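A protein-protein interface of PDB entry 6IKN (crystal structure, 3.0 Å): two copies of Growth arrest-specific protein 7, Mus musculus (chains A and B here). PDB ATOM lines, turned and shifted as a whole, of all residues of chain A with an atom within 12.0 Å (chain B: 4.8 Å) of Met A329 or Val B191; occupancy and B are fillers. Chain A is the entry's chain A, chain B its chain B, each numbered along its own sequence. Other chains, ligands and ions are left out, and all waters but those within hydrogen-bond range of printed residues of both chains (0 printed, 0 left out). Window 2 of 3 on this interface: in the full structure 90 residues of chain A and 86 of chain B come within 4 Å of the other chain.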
ATOM      1  N   ARG A 325     -16.233 -17.344 -30.265  1.00  0.00           N
ATOM      2  CA  ARG A 325     -15.122 -17.457 -29.332  1.00  0.00           C
ATOM      3  C   ARG A 325     -15.607 -17.552 -27.892  1.00  0.00           C
ATOM      4  O   ARG A 325     -16.696 -17.076 -27.569  1.00  0.00           O
ATOM      5  CB  ARG A 325     -14.174 -16.270 -29.508  1.00  0.00           C
ATOM      6  CG  ARG A 325     -13.312 -16.373 -30.756  1.00  0.00           C
ATOM      7  CD  ARG A 325     -12.272 -15.267 -30.812  1.00  0.00           C
ATOM      8  NE  ARG A 325     -12.870 -13.935 -30.740  1.00  0.00           N
ATOM      9  CZ  ARG A 325     -13.385 -13.288 -31.780  1.00  0.00           C
ATOM     10  NH1 ARG A 325     -13.393 -13.853 -32.980  1.00  0.00           N
ATOM     11  NH2 ARG A 325     -13.901 -12.078 -31.619  1.00  0.00           N
ATOM     12  N   PRO A 326     -14.800 -18.177 -27.022  1.00  0.00           N
ATOM     13  CA  PRO A 326     -15.148 -18.243 -25.603  1.00  0.00           C
ATOM     14  C   PRO A 326     -15.151 -16.873 -24.939  1.00  0.00           C
ATOM     15  O   PRO A 326     -14.541 -15.931 -25.442  1.00  0.00           O
ATOM     16  CB  PRO A 326     -14.044 -19.125 -25.007  1.00  0.00           C
ATOM     17  CG  PRO A 326     -13.495 -19.891 -26.163  1.00  0.00           C
ATOM     18  CD  PRO A 326     -13.589 -18.957 -27.329  1.00  0.00           C
ATOM     19  N   VAL A 327     -15.835 -16.779 -23.805  1.00  0.00           N
ATOM     20  CA  VAL A 327     -15.877 -15.554 -23.025  1.00  0.00           C
ATOM     21  C   VAL A 327     -15.704 -15.899 -21.556  1.00  0.00           C
ATOM     22  O   VAL A 327     -15.598 -17.068 -21.195  1.00  0.00           O
ATOM     23  CB  VAL A 327     -17.200 -14.793 -23.225  1.00  0.00           C
ATOM     24  CG1 VAL A 327     -17.311 -14.296 -24.652  1.00  0.00           C
ATOM     25  CG2 VAL A 327     -18.376 -15.688 -22.883  1.00  0.00           C
ATOM     26  N   ASP A 328     -15.680 -14.879 -20.707  1.00  0.00           N
ATOM     27  CA  ASP A 328     -15.476 -15.095 -19.283  1.00  0.00           C
ATOM     28  C   ASP A 328     -16.775 -15.549 -18.629  1.00  0.00           C
ATOM     29  O   ASP A 328     -17.860 -15.129 -19.030  1.00  0.00           O
ATOM     30  CB  ASP A 328     -14.954 -13.821 -18.608  1.00  0.00           C
ATOM     31  CG  ASP A 328     -13.493 -13.549 -18.913  1.00  0.00           C
ATOM     32  OD1 ASP A 328     -12.744 -14.516 -19.159  1.00  0.00           O
ATOM     33  OD2 ASP A 328     -13.089 -12.366 -18.896  1.00  0.00           O
ATOM     34  N   MET A 329     -16.669 -16.414 -17.627  1.00  0.00           N
ATOM     35  CA  MET A 329     -17.844 -16.826 -16.871  1.00  0.00           C
ATOM     36  C   MET A 329     -18.385 -15.620 -16.114  1.00  0.00           C
ATOM     37  O   MET A 329     -17.612 -14.877 -15.503  1.00  0.00           O
ATOM     38  CB  MET A 329     -17.501 -17.973 -15.917  1.00  0.00           C
ATOM     39  CG  MET A 329     -18.693 -18.555 -15.179  1.00  0.00           C
ATOM     40  SD  MET A 329     -18.412 -20.396 -14.560  1.00  0.00           S
ATOM     41  CE  MET A 329     -16.781 -20.198 -13.490  1.00  0.00           C
ATOM     42  N   GLU A 330     -19.704 -15.428 -16.185  1.00  0.00           N
ATOM     43  CA  GLU A 330     -20.377 -14.269 -15.603  1.00  0.00           C
ATOM     44  C   GLU A 330     -19.899 -12.974 -16.240  1.00  0.00           C
ATOM     45  O   GLU A 330     -20.636 -12.323 -16.979  1.00  0.00           O
ATOM     46  CB  GLU A 330     -20.166 -14.217 -14.089  1.00  0.00           C
ATOM     47  CG  GLU A 330     -20.728 -15.412 -13.349  1.00  0.00           C
ATOM     48  CD  GLU A 330     -20.832 -15.163 -11.857  1.00  0.00           C
ATOM     49  OE1 GLU A 330     -20.106 -14.278 -11.358  1.00  0.00           O
ATOM     50  OE2 GLU A 330     -21.644 -15.838 -11.186  1.00  0.00           O
ATOM     51  N   THR B  28     -24.480 -16.316 -20.133  1.00  0.00           N
ATOM     52  CA  THR B  28     -23.496 -17.092 -20.879  1.00  0.00           C
ATOM     53  C   THR B  28     -23.920 -18.557 -20.817  1.00  0.00           C
ATOM     54  O   THR B  28     -24.897 -18.887 -20.153  1.00  0.00           O
ATOM     55  CB  THR B  28     -22.068 -16.901 -20.334  1.00  0.00           C
ATOM     56  OG1 THR B  28     -21.976 -17.489 -19.030  1.00  0.00           O
ATOM     57  CG2 THR B  28     -21.719 -15.435 -20.264  1.00  0.00           C
ATOM     58  N   THR B  35     -17.086 -21.753 -21.884  1.00  0.00           N
ATOM     59  CA  THR B  35     -18.179 -20.782 -21.882  1.00  0.00           C
ATOM     60  C   THR B  35     -18.245 -19.944 -23.158  1.00  0.00           C
ATOM     61  O   THR B  35     -17.250 -19.369 -23.594  1.00  0.00           O
ATOM     62  CB  THR B  35     -18.087 -19.815 -20.682  1.00  0.00           C
ATOM     63  OG1 THR B  35     -16.945 -18.962 -20.840  1.00  0.00           O
ATOM     64  CG2 THR B  35     -17.959 -20.579 -19.381  1.00  0.00           C
ATOM     65  N   ARG B 187     -11.121 -27.032 -12.939  1.00  0.00           N
ATOM     66  CA  ARG B 187     -11.514 -25.718 -12.443  1.00  0.00           C
ATOM     67  C   ARG B 187     -13.032 -25.566 -12.420  1.00  0.00           C
ATOM     68  O   ARG B 187     -13.596 -25.046 -11.456  1.00  0.00           O
ATOM     69  CB  ARG B 187     -10.890 -24.615 -13.299  1.00  0.00           C
ATOM     70  CG  ARG B 187      -9.417 -24.379 -13.021  1.00  0.00           C
ATOM     71  CD  ARG B 187      -9.179 -24.017 -11.566  1.00  0.00           C
ATOM     72  NE  ARG B 187      -7.784 -23.673 -11.316  1.00  0.00           N
ATOM     73  CZ  ARG B 187      -6.838 -24.562 -11.037  1.00  0.00           C
ATOM     74  NH1 ARG B 187      -7.138 -25.851 -10.974  1.00  0.00           N
ATOM     75  NH2 ARG B 187      -5.594 -24.163 -10.820  1.00  0.00           N
ATOM     76  N   TYR B 188     -13.683 -26.024 -13.486  1.00  0.00           N
ATOM     77  CA  TYR B 188     -15.138 -25.957 -13.573  1.00  0.00           C
ATOM     78  C   TYR B 188     -15.766 -26.740 -12.423  1.00  0.00           C
ATOM     79  O   TYR B 188     -16.704 -26.265 -11.771  1.00  0.00           O
ATOM     80  CB  TYR B 188     -15.619 -26.500 -14.920  1.00  0.00           C
ATOM     81  CG  TYR B 188     -17.116 -26.432 -15.125  1.00  0.00           C
ATOM     82  CD1 TYR B 188     -17.723 -25.244 -15.506  1.00  0.00           C
ATOM     83  CD2 TYR B 188     -17.916 -27.556 -14.969  1.00  0.00           C
ATOM     84  CE1 TYR B 188     -19.088 -25.169 -15.706  1.00  0.00           C
ATOM     85  CE2 TYR B 188     -19.286 -27.492 -15.167  1.00  0.00           C
ATOM     86  CZ  TYR B 188     -19.864 -26.294 -15.538  1.00  0.00           C
ATOM     87  OH  TYR B 188     -21.224 -26.213 -15.741  1.00  0.00           O
ATOM     88  N   ALA B 189     -15.237 -27.937 -12.180  1.00  0.00           N
ATOM     89  CA  ALA B 189     -15.702 -28.784 -11.085  1.00  0.00           C
ATOM     90  C   ALA B 189     -15.605 -28.045  -9.752  1.00  0.00           C
ATOM     91  O   ALA B 189     -16.565 -28.017  -8.970  1.00  0.00           O
ATOM     92  CB  ALA B 189     -14.908 -30.080 -11.040  1.00  0.00           C
ATOM     93  N   SER B 190     -14.436 -27.461  -9.498  1.00  0.00           N
ATOM     94  CA  SER B 190     -14.206 -26.696  -8.277  1.00  0.00           C
ATOM     95  C   SER B 190     -15.241 -25.580  -8.143  1.00  0.00           C
ATOM     96  O   SER B 190     -15.802 -25.366  -7.066  1.00  0.00           O
ATOM     97  CB  SER B 190     -12.789 -26.118  -8.261  1.00  0.00           C
ATOM     98  OG  SER B 190     -12.610 -25.166  -9.300  1.00  0.00           O
ATOM     99  N   VAL B 191     -15.487 -24.883  -9.251  1.00  0.00           N
ATOM    100  CA  VAL B 191     -16.456 -23.792  -9.292  1.00  0.00           C
ATOM    101  C   VAL B 191     -17.849 -24.268  -8.887  1.00  0.00           C
ATOM    102  O   VAL B 191     -18.528 -23.627  -8.077  1.00  0.00           O
ATOM    103  CB  VAL B 191     -16.523 -23.161 -10.702  1.00  0.00           C
ATOM    104  CG1 VAL B 191     -17.833 -22.406 -10.897  1.00  0.00           C
ATOM    105  CG2 VAL B 191     -15.349 -22.224 -10.910  1.00  0.00           C
ATOM    106  N   GLU B 192     -18.267 -25.398  -9.449  1.00  0.00           N
ATOM    107  CA  GLU B 192     -19.586 -25.941  -9.158  1.00  0.00           C
ATOM    108  C   GLU B 192     -19.690 -26.320  -7.679  1.00  0.00           C
ATOM    109  O   GLU B 192     -20.708 -26.051  -7.025  1.00  0.00           O
ATOM    110  CB  GLU B 192     -19.875 -27.148 -10.049  1.00  0.00           C
ATOM    111  CG  GLU B 192     -20.122 -26.782 -11.508  1.00  0.00           C
ATOM    112  CD  GLU B 192     -21.119 -25.647 -11.671  1.00  0.00           C
ATOM    113  OE1 GLU B 192     -22.242 -25.757 -11.135  1.00  0.00           O
ATOM    114  OE2 GLU B 192     -20.773 -24.642 -12.330  1.00  0.00           O
ATOM    115  N   LYS B 193     -18.627 -26.930  -7.160  1.00  0.00           N
ATOM    116  CA  LYS B 193     -18.551 -27.275  -5.743  1.00  0.00           C
ATOM    117  C   LYS B 193     -18.756 -26.024  -4.891  1.00  0.00           C
ATOM    118  O   LYS B 193     -19.505 -26.033  -3.900  1.00  0.00           O
ATOM    119  CB  LYS B 193     -17.199 -27.920  -5.429  1.00  0.00           C
ATOM    120  CG  LYS B 193     -17.100 -28.581  -4.068  1.00  0.00           C
ATOM    121  CD  LYS B 193     -15.783 -29.334  -3.936  1.00  0.00           C
ATOM    122  CE  LYS B 193     -15.651 -29.990  -2.573  1.00  0.00           C
ATOM    123  NZ  LYS B 193     -16.803 -30.891  -2.284  1.00  0.00           N
ATOM    124  N   ALA B 194     -18.095 -24.943  -5.299  1.00  0.00           N
ATOM    125  CA  ALA B 194     -18.192 -23.669  -4.602  1.00  0.00           C
ATOM    126  C   ALA B 194     -19.628 -23.161  -4.625  1.00  0.00           C
ATOM    127  O   ALA B 194     -20.121 -22.626  -3.630  1.00  0.00           O
ATOM    128  CB  ALA B 194     -17.253 -22.648  -5.220  1.00  0.00           C
ATOM    129  N   ARG B 195     -20.293 -23.326  -5.766  1.00  0.00           N
ATOM    130  CA  ARG B 195     -21.681 -22.904  -5.911  1.00  0.00           C
ATOM    131  C   ARG B 195     -22.555 -23.652  -4.910  1.00  0.00           C
ATOM    132  O   ARG B 195     -23.417 -23.057  -4.245  1.00  0.00           O
ATOM    133  CB  ARG B 195     -22.159 -23.156  -7.342  1.00  0.00           C
ATOM    134  CG  ARG B 195     -21.838 -22.028  -8.309  1.00  0.00           C
ATOM    135  CD  ARG B 195     -22.482 -22.250  -9.668  1.00  0.00           C
ATOM    136  NE  ARG B 195     -22.336 -21.083 -10.533  1.00  0.00           N
ATOM    137  CZ  ARG B 195     -22.028 -21.142 -11.826  1.00  0.00           C
ATOM    138  NH1 ARG B 195     -21.834 -22.316 -12.411  1.00  0.00           N
ATOM    139  NH2 ARG B 195     -21.915 -20.025 -12.534  1.00  0.00           N
ATOM    140  N   LEU B 238     -16.389 -18.635  -4.001  1.00  0.00           N
ATOM    141  CA  LEU B 238     -16.984 -18.708  -5.333  1.00  0.00           C
ATOM    142  C   LEU B 238     -16.304 -17.762  -6.314  1.00  0.00           C
ATOM    143  O   LEU B 238     -15.887 -18.181  -7.397  1.00  0.00           O
ATOM    144  CB  LEU B 238     -18.478 -18.401  -5.285  1.00  0.00           C
ATOM    145  CG  LEU B 238     -19.145 -18.550  -6.653  1.00  0.00           C
ATOM    146  CD1 LEU B 238     -19.207 -20.009  -7.046  1.00  0.00           C
ATOM    147  CD2 LEU B 238     -20.535 -17.935  -6.653  1.00  0.00           C
ATOM    148  N   CYS B 241     -12.842 -19.160  -7.202  1.00  0.00           N
ATOM    149  CA  CYS B 241     -12.917 -20.311  -8.094  1.00  0.00           C
ATOM    150  C   CYS B 241     -13.264 -19.899  -9.523  1.00  0.00           C
ATOM    151  O   CYS B 241     -12.698 -20.431 -10.485  1.00  0.00           O
ATOM    152  CB  CYS B 241     -13.939 -21.322  -7.567  1.00  0.00           C
ATOM    153  SG  CYS B 241     -13.318 -22.379  -6.234  1.00  0.00           S
ATOM    154  N   VAL B 242     -14.181 -18.945  -9.655  1.00  0.00           N
ATOM    155  CA  VAL B 242     -14.556 -18.431 -10.967  1.00  0.00           C
ATOM    156  C   VAL B 242     -13.369 -17.743 -11.635  1.00  0.00           C
ATOM    157  O   VAL B 242     -13.132 -17.924 -12.832  1.00  0.00           O
ATOM    158  CB  VAL B 242     -15.735 -17.446 -10.877  1.00  0.00           C
ATOM    159  CG1 VAL B 242     -16.020 -16.825 -12.238  1.00  0.00           C
ATOM    160  CG2 VAL B 242     -16.971 -18.150 -10.350  1.00  0.00           C
ATOM    161  N   TYR B 245     -10.961 -20.313 -12.848  1.00  0.00           N
ATOM    162  CA  TYR B 245     -11.548 -20.930 -14.029  1.00  0.00           C
ATOM    163  C   TYR B 245     -11.271 -20.077 -15.259  1.00  0.00           C
ATOM    164  O   TYR B 245     -10.755 -20.569 -16.266  1.00  0.00           O
ATOM    165  CB  TYR B 245     -13.058 -21.122 -13.859  1.00  0.00           C
ATOM    166  CG  TYR B 245     -13.759 -21.507 -15.144  1.00  0.00           C
ATOM    167  CD1 TYR B 245     -13.834 -22.835 -15.545  1.00  0.00           C
ATOM    168  CD2 TYR B 245     -14.332 -20.542 -15.965  1.00  0.00           C
ATOM    169  CE1 TYR B 245     -14.466 -23.190 -16.717  1.00  0.00           C
ATOM    170  CE2 TYR B 245     -14.963 -20.890 -17.142  1.00  0.00           C
ATOM    171  CZ  TYR B 245     -15.028 -22.214 -17.512  1.00  0.00           C
ATOM    172  OH  TYR B 245     -15.657 -22.563 -18.684  1.00  0.00           O
ATOM    173  N   ASN B 246     -11.630 -18.799 -15.175  1.00  0.00           N
ATOM    174  CA  ASN B 246     -11.425 -17.875 -16.283  1.00  0.00           C
ATOM    175  C   ASN B 246      -9.963 -17.812 -16.719  1.00  0.00           C
ATOM    176  O   ASN B 246      -9.671 -17.723 -17.915  1.00  0.00           O
ATOM    177  CB  ASN B 246     -11.932 -16.481 -15.917  1.00  0.00           C
ATOM    178  CG  ASN B 246     -13.441 -16.376 -16.006  1.00  0.00           C
ATOM    179  OD1 ASN B 246     -14.079 -17.101 -16.770  1.00  0.00           O
ATOM    180  ND2 ASN B 246     -14.020 -15.465 -15.234  1.00  0.00           N
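Among the printed residues, merely in contact across the chains: Pro A326 with Thr B35, Met A329 with Tyr B245, Asp A328 with Asn B246, Met A329 with Val B191 and Met A329 with Val B242.
Of chain B, only Val B191, Val B242, Tyr B245 and Asn B246 come within 4 Å of Met A329. Val B191 touches one residue of chain A. No residue of chain A comes within 4 Å of Tyr B188. Ser B190 touches none of the printed residues of chain A. No residue of chain A comes within 4 Å of Glu B192. No residue of chain A comes within 4 Å of Arg B195. No residue of chain A comes within 4 Å of Leu B238. No residue of chain A comes within 4 Å of Cys B241. Val B242 touches one residue of chain A. Printed residues of chain A within 4 Å of Tyr B245: Met A329. Printed residues of chain A within 4 Å of Asn B246: Asp A328 and Met A329. Printed residues of chain B within 4 Å of Asp A328: Asn B246. Printed residues of chain B within 4 Å of Val A327: Thr B35. Of the printed residues of chain B, Pro A326 touches Thr B35 (3.1 Å). Lys B193 touches none of the printed residues of chain A. Thr B28 touches none of the printed residues of chain A. The nearest printed residue of chain B that does not touch Val A327 is Thr B28 (4.3 Å).
No position is printed for both chains. Of the 7 pairs that touch across the chains among the printed residues, none has its exchanged pair printed and touching as well.
The backbone NH (N) of Val A327 sits at hydrogen-bond distance from the backbone carbonyl oxygen (O) of Thr B35 (3.0 Å). The backbone NH (N) of Met A329 sits at hydrogen-bond distance from the side-chain amide oxygen (OD1) of Asn B246 (2.8 Å).
Of the 6 printed residues of chain A, 4 touch a printed residue of chain B. Hydrophobic or aromatic side chains of chain A that line the printed part of chain B: Pro A326, Val A327 and Met A329. Along chain A the printed residues that touch a printed residue of chain B span positions 326 to 329. Of the 16 printed residues of chain B, 5 touch a printed residue of chain A.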
